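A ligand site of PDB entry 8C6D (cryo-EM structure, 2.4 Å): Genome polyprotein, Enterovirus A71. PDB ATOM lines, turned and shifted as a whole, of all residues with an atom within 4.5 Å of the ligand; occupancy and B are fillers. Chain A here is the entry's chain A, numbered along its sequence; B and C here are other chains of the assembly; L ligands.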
ATOM      1  N   ILE A 111      17.318  10.838  21.335  1.00  0.00           N
ATOM      2  CA  ILE A 111      18.117  10.405  22.467  1.00  0.00           C
ATOM      3  C   ILE A 111      19.426   9.806  21.964  1.00  0.00           C
ATOM      4  O   ILE A 111      19.450   8.759  21.307  1.00  0.00           O
ATOM      5  CB  ILE A 111      17.364   9.425  23.352  1.00  0.00           C
ATOM      6  CG1 ILE A 111      16.078  10.064  23.859  1.00  0.00           C
ATOM      7  CG2 ILE A 111      18.240   9.065  24.501  1.00  0.00           C
ATOM      8  CD1 ILE A 111      15.065   9.073  24.384  1.00  0.00           C
ATOM      9  N   ASP A 112      20.525  10.478  22.281  1.00  0.00           N
ATOM     10  CA  ASP A 112      21.809  10.248  21.669  1.00  0.00           C
ATOM     11  C   ASP A 112      22.805  10.876  22.622  1.00  0.00           C
ATOM     12  O   ASP A 112      22.844  12.106  22.751  1.00  0.00           O
ATOM     13  CB  ASP A 112      21.832  10.878  20.255  1.00  0.00           C
ATOM     14  CG  ASP A 112      23.116  10.622  19.479  1.00  0.00           C
ATOM     15  OD1 ASP A 112      24.168  10.258  20.034  1.00  0.00           O
ATOM     16  OD2 ASP A 112      23.036  10.734  18.235  1.00  0.00           O
ATOM     17  N   ILE A 113      23.589  10.041  23.302  1.00  0.00           N
ATOM     18  CA  ILE A 113      24.496  10.502  24.355  1.00  0.00           C
ATOM     19  C   ILE A 113      25.864  10.794  23.757  1.00  0.00           C
ATOM     20  O   ILE A 113      26.814  11.118  24.484  1.00  0.00           O
ATOM     21  CB  ILE A 113      24.594   9.477  25.485  1.00  0.00           C
ATOM     22  CG1 ILE A 113      25.322   8.222  25.015  1.00  0.00           C
ATOM     23  CG2 ILE A 113      23.219   9.153  26.036  1.00  0.00           C
ATOM     24  CD1 ILE A 113      26.109   7.551  26.090  1.00  0.00           C
ATOM     25  N   THR A 114      25.974  10.699  22.438  1.00  0.00           N
ATOM     26  CA  THR A 114      27.203  11.002  21.733  1.00  0.00           C
ATOM     27  C   THR A 114      27.261  12.450  21.245  1.00  0.00           C
ATOM     28  O   THR A 114      28.041  12.745  20.334  1.00  0.00           O
ATOM     29  CB  THR A 114      27.398  10.037  20.553  1.00  0.00           C
ATOM     30  OG1 THR A 114      26.520  10.392  19.486  1.00  0.00           O
ATOM     31  CG2 THR A 114      27.121   8.607  20.983  1.00  0.00           C
ATOM     32  N   PHE A 131      23.421  -1.076  30.162  1.00  0.00           N
ATOM     33  CA  PHE A 131      23.319  -0.360  31.415  1.00  0.00           C
ATOM     34  C   PHE A 131      21.887   0.121  31.586  1.00  0.00           C
ATOM     35  O   PHE A 131      21.210   0.425  30.600  1.00  0.00           O
ATOM     36  CB  PHE A 131      24.287   0.834  31.481  1.00  0.00           C
ATOM     37  CG  PHE A 131      24.166   1.776  30.316  1.00  0.00           C
ATOM     38  CD1 PHE A 131      24.921   1.587  29.176  1.00  0.00           C
ATOM     39  CD2 PHE A 131      23.298   2.863  30.359  1.00  0.00           C
ATOM     40  CE1 PHE A 131      24.812   2.427  28.111  1.00  0.00           C
ATOM     41  CE2 PHE A 131      23.180   3.707  29.284  1.00  0.00           C
ATOM     42  CZ  PHE A 131      23.926   3.491  28.161  1.00  0.00           C
ATOM     43  N   PHE A 135      18.578   9.203  34.497  1.00  0.00           N
ATOM     44  CA  PHE A 135      18.537  10.424  33.701  1.00  0.00           C
ATOM     45  C   PHE A 135      18.051  11.561  34.586  1.00  0.00           C
ATOM     46  O   PHE A 135      16.950  11.505  35.127  1.00  0.00           O
ATOM     47  CB  PHE A 135      17.638  10.253  32.484  1.00  0.00           C
ATOM     48  CG  PHE A 135      18.368   9.804  31.259  1.00  0.00           C
ATOM     49  CD1 PHE A 135      18.611   8.462  31.027  1.00  0.00           C
ATOM     50  CD2 PHE A 135      18.800  10.729  30.323  1.00  0.00           C
ATOM     51  CE1 PHE A 135      19.279   8.059  29.892  1.00  0.00           C
ATOM     52  CE2 PHE A 135      19.465  10.334  29.194  1.00  0.00           C
ATOM     53  CZ  PHE A 135      19.705   8.995  28.975  1.00  0.00           C
ATOM     54  N   PHE A 137      17.332  15.695  34.640  1.00  0.00           N
ATOM     55  CA  PHE A 137      17.058  16.807  33.746  1.00  0.00           C
ATOM     56  C   PHE A 137      17.103  18.090  34.559  1.00  0.00           C
ATOM     57  O   PHE A 137      16.241  18.338  35.407  1.00  0.00           O
ATOM     58  CB  PHE A 137      15.708  16.625  33.067  1.00  0.00           C
ATOM     59  CG  PHE A 137      15.494  15.264  32.498  1.00  0.00           C
ATOM     60  CD1 PHE A 137      16.021  14.919  31.276  1.00  0.00           C
ATOM     61  CD2 PHE A 137      14.773  14.313  33.210  1.00  0.00           C
ATOM     62  CE1 PHE A 137      15.844  13.653  30.764  1.00  0.00           C
ATOM     63  CE2 PHE A 137      14.594  13.056  32.702  1.00  0.00           C
ATOM     64  CZ  PHE A 137      15.131  12.718  31.474  1.00  0.00           C
ATOM     65  N   TYR A 153       8.340  16.341  30.619  1.00  0.00           N
ATOM     66  CA  TYR A 153       9.434  15.596  30.007  1.00  0.00           C
ATOM     67  C   TYR A 153       8.883  14.270  29.523  1.00  0.00           C
ATOM     68  O   TYR A 153       8.800  13.318  30.294  1.00  0.00           O
ATOM     69  CB  TYR A 153      10.544  15.327  31.009  1.00  0.00           C
ATOM     70  CG  TYR A 153      11.246  16.527  31.520  1.00  0.00           C
ATOM     71  CD1 TYR A 153      11.437  17.649  30.725  1.00  0.00           C
ATOM     72  CD2 TYR A 153      11.728  16.546  32.809  1.00  0.00           C
ATOM     73  CE1 TYR A 153      12.089  18.743  31.209  1.00  0.00           C
ATOM     74  CE2 TYR A 153      12.380  17.633  33.301  1.00  0.00           C
ATOM     75  CZ  TYR A 153      12.558  18.723  32.495  1.00  0.00           C
ATOM     76  OH  TYR A 153      13.207  19.807  33.009  1.00  0.00           O
ATOM     77  N   MET A 154       8.522  14.184  28.253  1.00  0.00           N
ATOM     78  CA  MET A 154       7.972  12.940  27.740  1.00  0.00           C
ATOM     79  C   MET A 154       9.049  12.097  27.083  1.00  0.00           C
ATOM     80  O   MET A 154       9.699  12.534  26.132  1.00  0.00           O
ATOM     81  CB  MET A 154       6.832  13.187  26.759  1.00  0.00           C
ATOM     82  CG  MET A 154       6.108  11.901  26.418  1.00  0.00           C
ATOM     83  SD  MET A 154       4.411  12.177  25.947  1.00  0.00           S
ATOM     84  CE  MET A 154       4.687  13.197  24.522  1.00  0.00           C
ATOM     85  N   PHE A 155       9.243  10.895  27.605  1.00  0.00           N
ATOM     86  CA  PHE A 155       9.946   9.865  26.852  1.00  0.00           C
ATOM     87  C   PHE A 155       9.018   9.398  25.745  1.00  0.00           C
ATOM     88  O   PHE A 155       7.966   8.829  26.003  1.00  0.00           O
ATOM     89  CB  PHE A 155      10.347   8.710  27.769  1.00  0.00           C
ATOM     90  CG  PHE A 155      10.975   7.552  27.045  1.00  0.00           C
ATOM     91  CD1 PHE A 155      11.906   7.764  26.045  1.00  0.00           C
ATOM     92  CD2 PHE A 155      10.619   6.252  27.380  1.00  0.00           C
ATOM     93  CE1 PHE A 155      12.464   6.712  25.392  1.00  0.00           C
ATOM     94  CE2 PHE A 155      11.189   5.193  26.723  1.00  0.00           C
ATOM     95  CZ  PHE A 155      12.106   5.420  25.733  1.00  0.00           C
ATOM     96  N   PRO A 177       5.938   7.494  29.117  1.00  0.00           N
ATOM     97  CA  PRO A 177       6.383   8.044  30.397  1.00  0.00           C
ATOM     98  C   PRO A 177       6.602   9.539  30.267  1.00  0.00           C
ATOM     99  O   PRO A 177       7.320  10.004  29.374  1.00  0.00           O
ATOM    100  CB  PRO A 177       7.688   7.291  30.678  1.00  0.00           C
ATOM    101  CG  PRO A 177       7.773   6.231  29.648  1.00  0.00           C
ATOM    102  CD  PRO A 177       6.995   6.690  28.486  1.00  0.00           C
ATOM    103  N   SER A 178       5.965  10.298  31.151  1.00  0.00           N
ATOM    104  CA  SER A 178       6.183  11.725  31.228  1.00  0.00           C
ATOM    105  C   SER A 178       6.541  12.121  32.642  1.00  0.00           C
ATOM    106  O   SER A 178       6.046  11.542  33.610  1.00  0.00           O
ATOM    107  CB  SER A 178       4.975  12.540  30.787  1.00  0.00           C
ATOM    108  OG  SER A 178       4.877  12.545  29.383  1.00  0.00           O
ATOM    109  N   VAL A 179       7.423  13.109  32.756  1.00  0.00           N
ATOM    110  CA  VAL A 179       7.733  13.740  34.027  1.00  0.00           C
ATOM    111  C   VAL A 179       7.183  15.152  33.979  1.00  0.00           C
ATOM    112  O   VAL A 179       7.580  15.958  33.130  1.00  0.00           O
ATOM    113  CB  VAL A 179       9.236  13.744  34.319  1.00  0.00           C
ATOM    114  CG1 VAL A 179       9.513  14.657  35.493  1.00  0.00           C
ATOM    115  CG2 VAL A 179       9.683  12.367  34.656  1.00  0.00           C
ATOM    116  N   VAL A 190      15.025  10.330  36.820  1.00  0.00           N
ATOM    117  CA  VAL A 190      14.351   9.060  36.602  1.00  0.00           C
ATOM    118  C   VAL A 190      15.373   7.998  36.205  1.00  0.00           C
ATOM    119  O   VAL A 190      16.379   8.303  35.553  1.00  0.00           O
ATOM    120  CB  VAL A 190      13.261   9.170  35.514  1.00  0.00           C
ATOM    121  CG1 VAL A 190      12.025   9.852  36.052  1.00  0.00           C
ATOM    122  CG2 VAL A 190      13.784   9.885  34.288  1.00  0.00           C
ATOM    123  N   VAL A 192      15.977   5.082  33.738  1.00  0.00           N
ATOM    124  CA  VAL A 192      15.508   4.415  32.546  1.00  0.00           C
ATOM    125  C   VAL A 192      16.126   3.026  32.588  1.00  0.00           C
ATOM    126  O   VAL A 192      17.156   2.829  33.235  1.00  0.00           O
ATOM    127  CB  VAL A 192      15.857   5.221  31.280  1.00  0.00           C
ATOM    128  CG1 VAL A 192      15.523   6.679  31.505  1.00  0.00           C
ATOM    129  CG2 VAL A 192      17.288   5.022  30.879  1.00  0.00           C
ATOM    130  N   MET A 195      16.987  -0.458  27.465  1.00  0.00           N
ATOM    131  CA  MET A 195      15.793  -0.580  26.638  1.00  0.00           C
ATOM    132  C   MET A 195      16.067  -1.083  25.235  1.00  0.00           C
ATOM    133  O   MET A 195      15.182  -1.001  24.379  1.00  0.00           O
ATOM    134  CB  MET A 195      15.084   0.774  26.556  1.00  0.00           C
ATOM    135  CG  MET A 195      14.322   1.155  27.794  1.00  0.00           C
ATOM    136  SD  MET A 195      13.700   2.831  27.659  1.00  0.00           S
ATOM    137  CE  MET A 195      15.050   3.628  26.828  1.00  0.00           C
ATOM    138  N   TYR A 201      23.829  -1.782  24.204  1.00  0.00           N
ATOM    139  CA  TYR A 201      23.886  -0.664  23.290  1.00  0.00           C
ATOM    140  C   TYR A 201      25.174  -0.736  22.484  1.00  0.00           C
ATOM    141  O   TYR A 201      26.118  -1.430  22.842  1.00  0.00           O
ATOM    142  CB  TYR A 201      23.800   0.673  24.026  1.00  0.00           C
ATOM    143  CG  TYR A 201      22.472   0.930  24.692  1.00  0.00           C
ATOM    144  CD1 TYR A 201      21.299   0.960  23.959  1.00  0.00           C
ATOM    145  CD2 TYR A 201      22.406   1.137  26.066  1.00  0.00           C
ATOM    146  CE1 TYR A 201      20.093   1.209  24.576  1.00  0.00           C
ATOM    147  CE2 TYR A 201      21.200   1.387  26.683  1.00  0.00           C
ATOM    148  CZ  TYR A 201      20.051   1.409  25.934  1.00  0.00           C
ATOM    149  OH  TYR A 201      18.854   1.655  26.560  1.00  0.00           O
ATOM    150  N   TRP A 203      27.786   1.694  20.548  1.00  0.00           N
ATOM    151  CA  TRP A 203      28.358   2.956  20.121  1.00  0.00           C
ATOM    152  C   TRP A 203      29.058   2.851  18.782  1.00  0.00           C
ATOM    153  O   TRP A 203      29.344   3.860  18.155  1.00  0.00           O
ATOM    154  CB  TRP A 203      29.346   3.484  21.163  1.00  0.00           C
ATOM    155  CG  TRP A 203      28.961   3.158  22.532  1.00  0.00           C
ATOM    156  CD1 TRP A 203      29.614   2.331  23.382  1.00  0.00           C
ATOM    157  CD2 TRP A 203      27.799   3.606  23.240  1.00  0.00           C
ATOM    158  NE1 TRP A 203      28.969   2.254  24.573  1.00  0.00           N
ATOM    159  CE2 TRP A 203      27.839   3.038  24.516  1.00  0.00           C
ATOM    160  CE3 TRP A 203      26.741   4.458  22.915  1.00  0.00           C
ATOM    161  CZ2 TRP A 203      26.860   3.268  25.469  1.00  0.00           C
ATOM    162  CZ3 TRP A 203      25.772   4.695  23.862  1.00  0.00           C
ATOM    163  CH2 TRP A 203      25.840   4.098  25.119  1.00  0.00           C
ATOM    164  N   ASN A 228      20.292   1.264  19.129  1.00  0.00           N
ATOM    165  CA  ASN A 228      20.682   2.367  19.964  1.00  0.00           C
ATOM    166  C   ASN A 228      19.670   3.498  19.958  1.00  0.00           C
ATOM    167  O   ASN A 228      19.633   4.294  20.903  1.00  0.00           O
ATOM    168  CB  ASN A 228      22.028   2.908  19.503  1.00  0.00           C
ATOM    169  CG  ASN A 228      23.174   2.205  20.154  1.00  0.00           C
ATOM    170  OD1 ASN A 228      23.146   0.993  20.331  1.00  0.00           O
ATOM    171  ND2 ASN A 228      24.175   2.964  20.540  1.00  0.00           N
ATOM    172  N   MET A 230      16.731   4.863  20.933  1.00  0.00           N
ATOM    173  CA  MET A 230      15.768   4.558  21.964  1.00  0.00           C
ATOM    174  C   MET A 230      14.593   5.506  21.959  1.00  0.00           C
ATOM    175  O   MET A 230      13.740   5.421  22.843  1.00  0.00           O
ATOM    176  CB  MET A 230      16.450   4.546  23.325  1.00  0.00           C
ATOM    177  CG  MET A 230      17.443   3.409  23.459  1.00  0.00           C
ATOM    178  SD  MET A 230      16.647   1.797  23.401  1.00  0.00           S
ATOM    179  CE  MET A 230      17.048   1.193  21.762  1.00  0.00           C
ATOM    180  N   PHE A 233      13.409  12.111  23.355  1.00  0.00           N
ATOM    181  CA  PHE A 233      13.068  12.798  24.591  1.00  0.00           C
ATOM    182  C   PHE A 233      12.333  14.078  24.225  1.00  0.00           C
ATOM    183  O   PHE A 233      12.895  14.951  23.562  1.00  0.00           O
ATOM    184  CB  PHE A 233      14.312  13.109  25.418  1.00  0.00           C
ATOM    185  CG  PHE A 233      14.013  13.946  26.614  1.00  0.00           C
ATOM    186  CD1 PHE A 233      13.331  13.405  27.686  1.00  0.00           C
ATOM    187  CD2 PHE A 233      14.376  15.277  26.654  1.00  0.00           C
ATOM    188  CE1 PHE A 233      13.039  14.180  28.777  1.00  0.00           C
ATOM    189  CE2 PHE A 233      14.084  16.051  27.745  1.00  0.00           C
ATOM    190  CZ  PHE A 233      13.416  15.496  28.808  1.00  0.00           C
ATOM    191  N   MET A 253      22.956  12.050  32.432  1.00  0.00           N
ATOM    192  CA  MET A 253      22.733  10.614  32.457  1.00  0.00           C
ATOM    193  C   MET A 253      23.770   9.958  33.357  1.00  0.00           C
ATOM    194  O   MET A 253      24.977  10.086  33.115  1.00  0.00           O
ATOM    195  CB  MET A 253      22.788  10.009  31.060  1.00  0.00           C
ATOM    196  CG  MET A 253      22.639   8.521  31.064  1.00  0.00           C
ATOM    197  SD  MET A 253      23.157   7.717  29.546  1.00  0.00           S
ATOM    198  CE  MET A 253      24.849   8.250  29.507  1.00  0.00           C
ATOM    199  N   ILE B  24      10.876   4.821  34.812  1.00  0.00           N
ATOM    200  CA  ILE B  24       9.947   5.343  33.823  1.00  0.00           C
ATOM    201  C   ILE B  24       9.054   4.272  33.210  1.00  0.00           C
ATOM    202  O   ILE B  24       8.063   4.604  32.563  1.00  0.00           O
ATOM    203  CB  ILE B  24      10.674   6.050  32.672  1.00  0.00           C
ATOM    204  CG1 ILE B  24      11.787   5.151  32.111  1.00  0.00           C
ATOM    205  CG2 ILE B  24      11.194   7.363  33.109  1.00  0.00           C
ATOM    206  CD1 ILE B  24      12.078   5.388  30.653  1.00  0.00           C
ATOM    207  N   LEU C  14       6.207  11.874  37.717  1.00  0.00           N
ATOM    208  CA  LEU C  14       6.395  10.842  36.723  1.00  0.00           C
ATOM    209  C   LEU C  14       5.058  10.137  36.520  1.00  0.00           C
ATOM    210  O   LEU C  14       4.468   9.632  37.487  1.00  0.00           O
ATOM    211  CB  LEU C  14       7.483   9.852  37.134  1.00  0.00           C
ATOM    212  CG  LEU C  14       7.646   8.655  36.207  1.00  0.00           C
ATOM    213  CD1 LEU C  14       8.052   9.072  34.805  1.00  0.00           C
ATOM    214  CD2 LEU C  14       8.658   7.688  36.754  1.00  0.00           C
HETATM  215  C1  LIG L   1      22.524   5.067  22.446  1.00  0.00           C
HETATM  216  C2  LIG L   1      22.057   4.711  23.717  1.00  0.00           C
HETATM  217  C3  LIG L   1      21.328   5.693  24.619  1.00  0.00           C
HETATM  218  C4  LIG L   1      20.881   4.974  25.955  1.00  0.00           C
HETATM  219  C5  LIG L   1      20.119   5.905  26.991  1.00  0.00           C
HETATM  220  C6  LIG L   1      17.522   6.462  26.853  1.00  0.00           C
HETATM  221  C7  LIG L   1      14.492   8.568  28.452  1.00  0.00           C
HETATM  222  C8  LIG L   1      13.108   9.924  30.249  1.00  0.00           C
HETATM  223  C9  LIG L   1      11.155  11.259  31.376  1.00  0.00           C
HETATM  224  O1  LIG L   1      23.333   7.292  22.543  1.00  0.00           O
HETATM  225  C10 LIG L   1      22.323   6.471  21.881  1.00  0.00           C
HETATM  226  C11 LIG L   1      22.588   6.434  20.304  1.00  0.00           C
HETATM  227  N1  LIG L   1      21.905   7.518  19.558  1.00  0.00           N
HETATM  228  C12 LIG L   1      24.137   6.491  20.049  1.00  0.00           C
HETATM  229  O2  LIG L   1      24.266   5.998  18.647  1.00  0.00           O
HETATM  230  C13 LIG L   1      18.640   5.463  27.345  1.00  0.00           C
HETATM  231  C14 LIG L   1      16.409   6.864  27.884  1.00  0.00           C
HETATM  232  C15 LIG L   1      15.949   8.358  27.897  1.00  0.00           C
HETATM  233  C16 LIG L   1      14.212   9.949  29.138  1.00  0.00           C
HETATM  234  C17 LIG L   1      12.000  11.022  30.107  1.00  0.00           C
HETATM  235  C18 LIG L   1       9.870  10.413  31.455  1.00  0.00           C
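N of Ile 113 sits at hydrogen-bond distance from O1 of the ligand, at 2.9 Å.
O of Ile 111 sits at hydrogen-bond distance from N1 of the ligand, at 3.3 Å.
OD1 of Asp 112 lies within salt-bridge range of N1 of the ligand (3.6 Å).
The backbone carbonyl oxygen (O) of Val 179 is in hydrogen-bond range of the backbone NH (N) of Tyr 153 (2.7 Å).
O of Pro 177 is in hydrogen-bond range of N of Phe 155 (2.8 Å).
The side-chain carboxylate (OD1) of Asp 112 sits at hydrogen-bond distance from the side-chain hydroxyl (OG1) of Thr 114 (2.4 Å).
The side-chain hydroxyl of Tyr 201 sits at hydrogen-bond distance from the backbone NH of Met 195.
N of Phe 135 lies within hydrogen-bond range of O of Val 190, 2.6 Å away.
The side-chain sulfur (SD) of Met 154 lies close to the side-chain hydroxyl (OG) of Ser 178, at 3.5 Å.
Merely in contact with the ligand: Asn 228 (3.3 Å), Tyr 153 (3.3 Å), Pro 177 (3.3 Å), Trp 203 (3.6 Å), Phe 233 (3.6 Å), Phe 155 (3.6 Å), Val 192 (3.6 Å), Tyr 201 (3.7 Å), Phe 137 (3.7 Å), Met 195 (3.7 Å), Phe 135 (3.7 Å), Ile 24 of chain B (3.7 Å), Val 179 (3.8 Å), Thr 114 (3.8 Å) and Ser 178 (3.9 Å).
Of the 24 residues printed, 18 come within 4 Å of the ligand.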
